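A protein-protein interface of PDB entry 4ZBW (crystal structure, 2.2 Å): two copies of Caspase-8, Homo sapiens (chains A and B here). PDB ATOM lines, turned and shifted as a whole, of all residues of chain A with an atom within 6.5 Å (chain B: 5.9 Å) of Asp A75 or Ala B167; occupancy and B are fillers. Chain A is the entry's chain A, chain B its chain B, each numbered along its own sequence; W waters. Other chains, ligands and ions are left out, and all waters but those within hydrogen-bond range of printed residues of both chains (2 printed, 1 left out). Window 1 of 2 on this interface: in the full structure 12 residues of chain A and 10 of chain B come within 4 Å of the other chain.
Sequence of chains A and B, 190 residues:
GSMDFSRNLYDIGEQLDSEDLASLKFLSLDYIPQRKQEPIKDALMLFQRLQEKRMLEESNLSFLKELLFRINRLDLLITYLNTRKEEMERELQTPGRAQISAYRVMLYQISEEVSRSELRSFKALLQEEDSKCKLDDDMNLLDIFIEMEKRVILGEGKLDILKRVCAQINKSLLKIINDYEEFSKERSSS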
ATOM      1  N   GLN A  15     -25.061  23.267  -1.345  1.00  0.00           N
ATOM      2  CA  GLN A  15     -24.465  22.435  -2.368  1.00  0.00           C
ATOM      3  C   GLN A  15     -23.640  23.277  -3.325  1.00  0.00           C
ATOM      4  O   GLN A  15     -22.900  22.750  -4.152  1.00  0.00           O
ATOM      5  CB  GLN A  15     -25.548  21.667  -3.119  1.00  0.00           C
ATOM      6  CG  GLN A  15     -26.454  20.846  -2.209  1.00  0.00           C
ATOM      7  CD  GLN A  15     -25.695  19.828  -1.378  1.00  0.00           C
ATOM      8  OE1 GLN A  15     -24.660  19.306  -1.797  1.00  0.00           O
ATOM      9  NE2 GLN A  15     -26.207  19.545  -0.187  1.00  0.00           N
ATOM     10  N   ASN A  72     -24.851  25.391 -14.813  1.00  0.00           N
ATOM     11  CA  ASN A  72     -24.875  23.947 -15.052  1.00  0.00           C
ATOM     12  C   ASN A  72     -25.042  23.089 -13.795  1.00  0.00           C
ATOM     13  O   ASN A  72     -24.509  21.981 -13.720  1.00  0.00           O
ATOM     14  CB  ASN A  72     -23.600  23.520 -15.794  1.00  0.00           C
ATOM     15  CG  ASN A  72     -23.758  22.190 -16.514  1.00  0.00           C
ATOM     16  OD1 ASN A  72     -24.850  21.838 -16.965  1.00  0.00           O
ATOM     17  ND2 ASN A  72     -22.665  21.441 -16.617  1.00  0.00           N
ATOM     18  N   ARG A  73     -25.783  23.587 -12.808  1.00  0.00           N
ATOM     19  CA  ARG A  73     -26.103  22.766 -11.644  1.00  0.00           C
ATOM     20  C   ARG A  73     -27.430  22.042 -11.861  1.00  0.00           C
ATOM     21  O   ARG A  73     -28.381  22.234 -11.104  1.00  0.00           O
ATOM     22  CB  ARG A  73     -26.158  23.606 -10.361  1.00  0.00           C
ATOM     23  CG  ARG A  73     -24.803  24.141  -9.891  1.00  0.00           C
ATOM     24  CD  ARG A  73     -23.748  23.039  -9.811  1.00  0.00           C
ATOM     25  NE  ARG A  73     -24.125  21.953  -8.910  1.00  0.00           N
ATOM     26  CZ  ARG A  73     -23.760  21.870  -7.633  1.00  0.00           C
ATOM     27  NH1 ARG A  73     -22.992  22.808  -7.091  1.00  0.00           N
ATOM     28  NH2 ARG A  73     -24.154  20.839  -6.898  1.00  0.00           N
ATOM     29  N   LEU A  74     -27.479  21.208 -12.899  1.00  0.00           N
ATOM     30  CA  LEU A  74     -28.688  20.465 -13.255  1.00  0.00           C
ATOM     31  C   LEU A  74     -29.104  19.510 -12.139  1.00  0.00           C
ATOM     32  O   LEU A  74     -30.297  19.225 -11.950  1.00  0.00           O
ATOM     33  CB  LEU A  74     -28.470  19.689 -14.559  1.00  0.00           C
ATOM     34  CG  LEU A  74     -27.970  20.503 -15.756  1.00  0.00           C
ATOM     35  CD1 LEU A  74     -27.744  19.612 -16.977  1.00  0.00           C
ATOM     36  CD2 LEU A  74     -28.940  21.637 -16.081  1.00  0.00           C
ATOM     37  N   ASP A  75     -28.113  19.029 -11.396  1.00  0.00           N
ATOM     38  CA  ASP A  75     -28.362  18.152 -10.261  1.00  0.00           C
ATOM     39  C   ASP A  75     -29.215  18.850  -9.197  1.00  0.00           C
ATOM     40  O   ASP A  75     -30.124  18.248  -8.623  1.00  0.00           O
ATOM     41  CB  ASP A  75     -27.036  17.668  -9.660  1.00  0.00           C
ATOM     42  CG  ASP A  75     -26.108  18.812  -9.280  1.00  0.00           C
ATOM     43  OD1 ASP A  75     -26.130  19.859  -9.962  1.00  0.00           O
ATOM     44  OD2 ASP A  75     -25.352  18.665  -8.296  1.00  0.00           O
ATOM     45  N   LEU A  76     -28.933  20.126  -8.953  1.00  0.00           N
ATOM     46  CA  LEU A  76     -29.663  20.880  -7.940  1.00  0.00           C
ATOM     47  C   LEU A  76     -31.055  21.239  -8.434  1.00  0.00           C
ATOM     48  O   LEU A  76     -32.013  21.237  -7.662  1.00  0.00           O
ATOM     49  CB  LEU A  76     -28.901  22.148  -7.556  1.00  0.00           C
ATOM     50  CG  LEU A  76     -27.530  21.913  -6.927  1.00  0.00           C
ATOM     51  CD1 LEU A  76     -26.943  23.220  -6.409  1.00  0.00           C
ATOM     52  CD2 LEU A  76     -27.634  20.877  -5.824  1.00  0.00           C
ATOM     53  N   LEU A  77     -31.161  21.532  -9.727  1.00  0.00           N
ATOM     54  CA  LEU A  77     -32.452  21.813 -10.338  1.00  0.00           C
ATOM     55  C   LEU A  77     -33.375  20.619 -10.157  1.00  0.00           C
ATOM     56  O   LEU A  77     -34.523  20.771  -9.719  1.00  0.00           O
ATOM     57  CB  LEU A  77     -32.292  22.146 -11.822  1.00  0.00           C
ATOM     58  CG  LEU A  77     -31.834  23.573 -12.128  1.00  0.00           C
ATOM     59  CD1 LEU A  77     -31.414  23.707 -13.582  1.00  0.00           C
ATOM     60  CD2 LEU A  77     -32.939  24.571 -11.787  1.00  0.00           C
ATOM     61  N   ILE A  78     -32.856  19.428 -10.457  1.00  0.00           N
ATOM     62  CA  ILE A  78     -33.635  18.206 -10.280  1.00  0.00           C
ATOM     63  C   ILE A  78     -33.972  17.955  -8.811  1.00  0.00           C
ATOM     64  O   ILE A  78     -35.139  17.802  -8.455  1.00  0.00           O
ATOM     65  CB  ILE A  78     -32.895  16.968 -10.826  1.00  0.00           C
ATOM     66  CG1 ILE A  78     -32.768  17.047 -12.346  1.00  0.00           C
ATOM     67  CG2 ILE A  78     -33.625  15.692 -10.422  1.00  0.00           C
ATOM     68  CD1 ILE A  78     -31.941  15.933 -12.948  1.00  0.00           C
ATOM     69  N   THR A  79     -32.945  17.923  -7.965  1.00  0.00           N
ATOM     70  CA  THR A  79     -33.120  17.556  -6.561  1.00  0.00           C
ATOM     71  C   THR A  79     -34.050  18.495  -5.791  1.00  0.00           C
ATOM     72  O   THR A  79     -34.978  18.048  -5.115  1.00  0.00           O
ATOM     73  CB  THR A  79     -31.767  17.511  -5.828  1.00  0.00           C
ATOM     74  OG1 THR A  79     -30.914  16.543  -6.451  1.00  0.00           O
ATOM     75  CG2 THR A  79     -31.961  17.138  -4.362  1.00  0.00           C
ATOM     76  N   TYR A  80     -33.805  19.795  -5.896  1.00  0.00           N
ATOM     77  CA  TYR A  80     -34.489  20.749  -5.034  1.00  0.00           C
ATOM     78  C   TYR A  80     -35.557  21.579  -5.740  1.00  0.00           C
ATOM     79  O   TYR A  80     -36.403  22.182  -5.079  1.00  0.00           O
ATOM     80  CB  TYR A  80     -33.469  21.679  -4.376  1.00  0.00           C
ATOM     81  CG  TYR A  80     -32.481  20.950  -3.496  1.00  0.00           C
ATOM     82  CD1 TYR A  80     -32.865  20.443  -2.260  1.00  0.00           C
ATOM     83  CD2 TYR A  80     -31.163  20.775  -3.893  1.00  0.00           C
ATOM     84  CE1 TYR A  80     -31.966  19.774  -1.451  1.00  0.00           C
ATOM     85  CE2 TYR A  80     -30.257  20.110  -3.091  1.00  0.00           C
ATOM     86  CZ  TYR A  80     -30.663  19.612  -1.870  1.00  0.00           C
ATOM     87  OH  TYR A  80     -29.763  18.949  -1.068  1.00  0.00           O
ATOM     88  N   LEU B 162     -21.576  10.417 -20.727  1.00  0.00           N
ATOM     89  CA  LEU B 162     -21.138  10.286 -19.343  1.00  0.00           C
ATOM     90  C   LEU B 162     -21.309  11.608 -18.593  1.00  0.00           C
ATOM     91  O   LEU B 162     -21.830  11.638 -17.474  1.00  0.00           O
ATOM     92  CB  LEU B 162     -19.678   9.826 -19.279  1.00  0.00           C
ATOM     93  CG  LEU B 162     -19.063   9.729 -17.880  1.00  0.00           C
ATOM     94  CD1 LEU B 162     -19.715   8.615 -17.073  1.00  0.00           C
ATOM     95  CD2 LEU B 162     -17.551   9.546 -17.945  1.00  0.00           C
ATOM     96  N   LYS B 163     -20.890  12.700 -19.225  1.00  0.00           N
ATOM     97  CA  LYS B 163     -20.984  14.019 -18.610  1.00  0.00           C
ATOM     98  C   LYS B 163     -22.422  14.513 -18.499  1.00  0.00           C
ATOM     99  O   LYS B 163     -22.792  15.105 -17.490  1.00  0.00           O
ATOM    100  CB  LYS B 163     -20.150  15.038 -19.386  1.00  0.00           C
ATOM    101  CG  LYS B 163     -18.658  14.884 -19.173  1.00  0.00           C
ATOM    102  CD  LYS B 163     -17.913  16.158 -19.527  1.00  0.00           C
ATOM    103  CE  LYS B 163     -17.503  16.165 -20.984  1.00  0.00           C
ATOM    104  NZ  LYS B 163     -16.718  17.384 -21.323  1.00  0.00           N
ATOM    105  N   ARG B 164     -23.228  14.279 -19.531  1.00  0.00           N
ATOM    106  CA  ARG B 164     -24.619  14.712 -19.502  1.00  0.00           C
ATOM    107  C   ARG B 164     -25.389  13.993 -18.403  1.00  0.00           C
ATOM    108  O   ARG B 164     -26.252  14.582 -17.755  1.00  0.00           O
ATOM    109  CB  ARG B 164     -25.293  14.490 -20.857  1.00  0.00           C
ATOM    110  CG  ARG B 164     -24.874  15.494 -21.914  1.00  0.00           C
ATOM    111  CD  ARG B 164     -25.912  15.610 -23.019  1.00  0.00           C
ATOM    112  NE  ARG B 164     -26.049  14.380 -23.793  1.00  0.00           N
ATOM    113  CZ  ARG B 164     -25.325  14.094 -24.872  1.00  0.00           C
ATOM    114  NH1 ARG B 164     -24.407  14.950 -25.302  1.00  0.00           N
ATOM    115  NH2 ARG B 164     -25.518  12.952 -25.520  1.00  0.00           N
ATOM    116  N   VAL B 165     -25.066  12.723 -18.184  1.00  0.00           N
ATOM    117  CA  VAL B 165     -25.671  11.985 -17.084  1.00  0.00           C
ATOM    118  C   VAL B 165     -25.167  12.506 -15.734  1.00  0.00           C
ATOM    119  O   VAL B 165     -25.964  12.884 -14.870  1.00  0.00           O
ATOM    120  CB  VAL B 165     -25.382  10.470 -17.193  1.00  0.00           C
ATOM    121  CG1 VAL B 165     -25.831   9.745 -15.931  1.00  0.00           C
ATOM    122  CG2 VAL B 165     -26.066   9.887 -18.423  1.00  0.00           C
ATOM    123  N   CYS B 166     -23.846  12.553 -15.569  1.00  0.00           N
ATOM    124  CA  CYS B 166     -23.247  12.923 -14.285  1.00  0.00           C
ATOM    125  C   CYS B 166     -23.582  14.346 -13.832  1.00  0.00           C
ATOM    126  O   CYS B 166     -23.681  14.611 -12.634  1.00  0.00           O
ATOM    127  CB  CYS B 166     -21.729  12.753 -14.347  1.00  0.00           C
ATOM    128  SG  CYS B 166     -21.199  11.033 -14.275  1.00  0.00           S
ATOM    129  N   ALA B 167     -23.763  15.254 -14.784  1.00  0.00           N
ATOM    130  CA  ALA B 167     -24.084  16.642 -14.464  1.00  0.00           C
ATOM    131  C   ALA B 167     -25.431  16.756 -13.753  1.00  0.00           C
ATOM    132  O   ALA B 167     -25.662  17.691 -12.990  1.00  0.00           O
ATOM    133  CB  ALA B 167     -24.085  17.491 -15.725  1.00  0.00           C
ATOM    134  N   GLN B 168     -26.309  15.790 -13.998  1.00  0.00           N
ATOM    135  CA  GLN B 168     -27.650  15.816 -13.433  1.00  0.00           C
ATOM    136  C   GLN B 168     -27.718  15.060 -12.111  1.00  0.00           C
ATOM    137  O   GLN B 168     -28.768  15.007 -11.470  1.00  0.00           O
ATOM    138  CB  GLN B 168     -28.656  15.226 -14.422  1.00  0.00           C
ATOM    139  CG  GLN B 168     -28.623  15.865 -15.797  1.00  0.00           C
ATOM    140  CD  GLN B 168     -29.628  15.244 -16.751  1.00  0.00           C
ATOM    141  OE1 GLN B 168     -30.836  15.461 -16.628  1.00  0.00           O
ATOM    142  NE2 GLN B 168     -29.136  14.454 -17.699  1.00  0.00           N
ATOM    143  N   ILE B 169     -26.592  14.486 -11.702  1.00  0.00           N
ATOM    144  CA  ILE B 169     -26.542  13.699 -10.475  1.00  0.00           C
ATOM    145  C   ILE B 169     -25.792  14.431  -9.368  1.00  0.00           C
ATOM    146  O   ILE B 169     -26.339  14.680  -8.292  1.00  0.00           O
ATOM    147  CB  ILE B 169     -25.875  12.330 -10.714  1.00  0.00           C
ATOM    148  CG1 ILE B 169     -26.660  11.533 -11.757  1.00  0.00           C
ATOM    149  CG2 ILE B 169     -25.777  11.550  -9.415  1.00  0.00           C
ATOM    150  CD1 ILE B 169     -26.043  10.189 -12.097  1.00  0.00           C
ATOM    151  N   ASN B 170     -24.538  14.775  -9.639  1.00  0.00           N
ATOM    152  CA  ASN B 170     -23.694  15.429  -8.649  1.00  0.00           C
ATOM    153  C   ASN B 170     -22.505  16.118  -9.307  1.00  0.00           C
ATOM    154  O   ASN B 170     -21.791  15.506 -10.107  1.00  0.00           O
ATOM    155  CB  ASN B 170     -23.211  14.411  -7.615  1.00  0.00           C
ATOM    156  CG  ASN B 170     -22.790  15.058  -6.310  1.00  0.00           C
ATOM    157  OD1 ASN B 170     -22.149  16.110  -6.299  1.00  0.00           O
ATOM    158  ND2 ASN B 170     -23.154  14.430  -5.198  1.00  0.00           N
ATOM    159  N   LYS B 171     -22.290  17.386  -8.960  1.00  0.00           N
ATOM    160  CA  LYS B 171     -21.214  18.179  -9.555  1.00  0.00           C
ATOM    161  C   LYS B 171     -19.835  17.551  -9.337  1.00  0.00           C
ATOM    162  O   LYS B 171     -18.940  17.714 -10.165  1.00  0.00           O
ATOM    163  CB  LYS B 171     -21.222  19.607  -8.996  1.00  0.00           C
ATOM    164  CG  LYS B 171     -20.156  20.506  -9.614  1.00  0.00           C
ATOM    165  CD  LYS B 171     -20.095  21.884  -8.974  1.00  0.00           C
ATOM    166  CE  LYS B 171     -19.015  22.723  -9.645  1.00  0.00           C
ATOM    167  NZ  LYS B 171     -18.907  24.090  -9.080  1.00  0.00           N
ATOM    168  N   LEU B 174     -18.858  15.219 -12.149  1.00  0.00           N
ATOM    169  CA  LEU B 174     -18.549  16.029 -13.313  1.00  0.00           C
ATOM    170  C   LEU B 174     -17.174  16.662 -13.160  1.00  0.00           C
ATOM    171  O   LEU B 174     -16.472  16.877 -14.142  1.00  0.00           O
ATOM    172  CB  LEU B 174     -19.618  17.105 -13.508  1.00  0.00           C
ATOM    173  CG  LEU B 174     -19.547  17.926 -14.793  1.00  0.00           C
ATOM    174  CD1 LEU B 174     -19.707  17.011 -15.997  1.00  0.00           C
ATOM    175  CD2 LEU B 174     -20.609  19.012 -14.790  1.00  0.00           C
HETATM  176  O   HOH W   1     -29.916  15.232  -8.967  1.00  0.00           O
HETATM  177  O   HOH W   2     -26.065  17.275  -6.081  1.00  0.00           O
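N of Lys B171 is in hydrogen-bond range of OD2 of Asp A75, 3.4 Å away.
N of Asp A75 lies within hydrogen-bond range of O of Ala B167, at 3.2 Å.
OG1 of Thr A79 is in hydrogen-bond range of O of Asp A75, 2.9 Å away.
O of Arg B164 lies within hydrogen-bond range of NE2 of Gln B168 (2.9 Å).
The backbone carbonyl oxygen of Gln A15 lies within hydrogen-bond range of the guanidinium group of Arg A73.
NH2 of Arg A73 is in salt-bridge range of OD2 of Asp A75 (2.8 Å).
Among the printed residues, pairs that only touch across the chains: Asn A72 with Leu B174 (3.7 Å), Arg A73 with Lys B171 (3.6 Å), Leu A74 with Ala B167 (3.8 Å), Asp A75 with Gln B168 (3.4 Å), Asp A75 with Ile B169 (3.4 Å), Asp A75 with Asn B170 (3.7 Å) and Ile A78 with Gln B168 (3.6 Å).
Of the printed residues of chain B, Arg A73 touches Lys B171 (3.6 Å).
Asp A75 touches five residues of chain B.
Printed residues of chain B within 4 Å of Ile A78: Gln B168.
Val B165 touches none of the printed residues of chain A.
Printed residues of chain A within 4 Å of Lys B171: Arg A73 and Asp A75.
Printed residues of chain A within 4 Å of Leu B174: Asn A72.
The nearest printed residue of chain B that does not touch Ile A78 is Ile B169 (5.7 Å).
Hydrophobic or aromatic side chains of chain B that line the printed part of chain A: Leu B174.
Along chain B the printed residues that touch a printed residue of chain A span positions 167 to 174.
Printed residues of chain A that touch a printed residue of chain B: Asn A72, Arg A73, Leu A74, Asp A75 and Ile A78.
Hydrophobic or aromatic side chains of chain A within 4 Å of the printed part of chain B: Leu A74 and Ile A78.
Among the printed residues, 9 pairs touch across the chains.
No position is printed for both chains.
Of the 9 pairs that touch across the chains among the printed residues, none has its exchanged pair printed and touching as well.
Water W2 lies within hydrogen-bond range of OD2 of Asp A75 (2.7 Å) and O of Ile B169 (3.4 Å).
Water W1 lies within hydrogen-bond range of the backbone carbonyl oxygen of Gln B168 (2.8 Å), the side-chain hydroxyl of Thr A79 (3.0 Å) and the backbone carbonyl oxygen of Asp A75 (3.0 Å).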
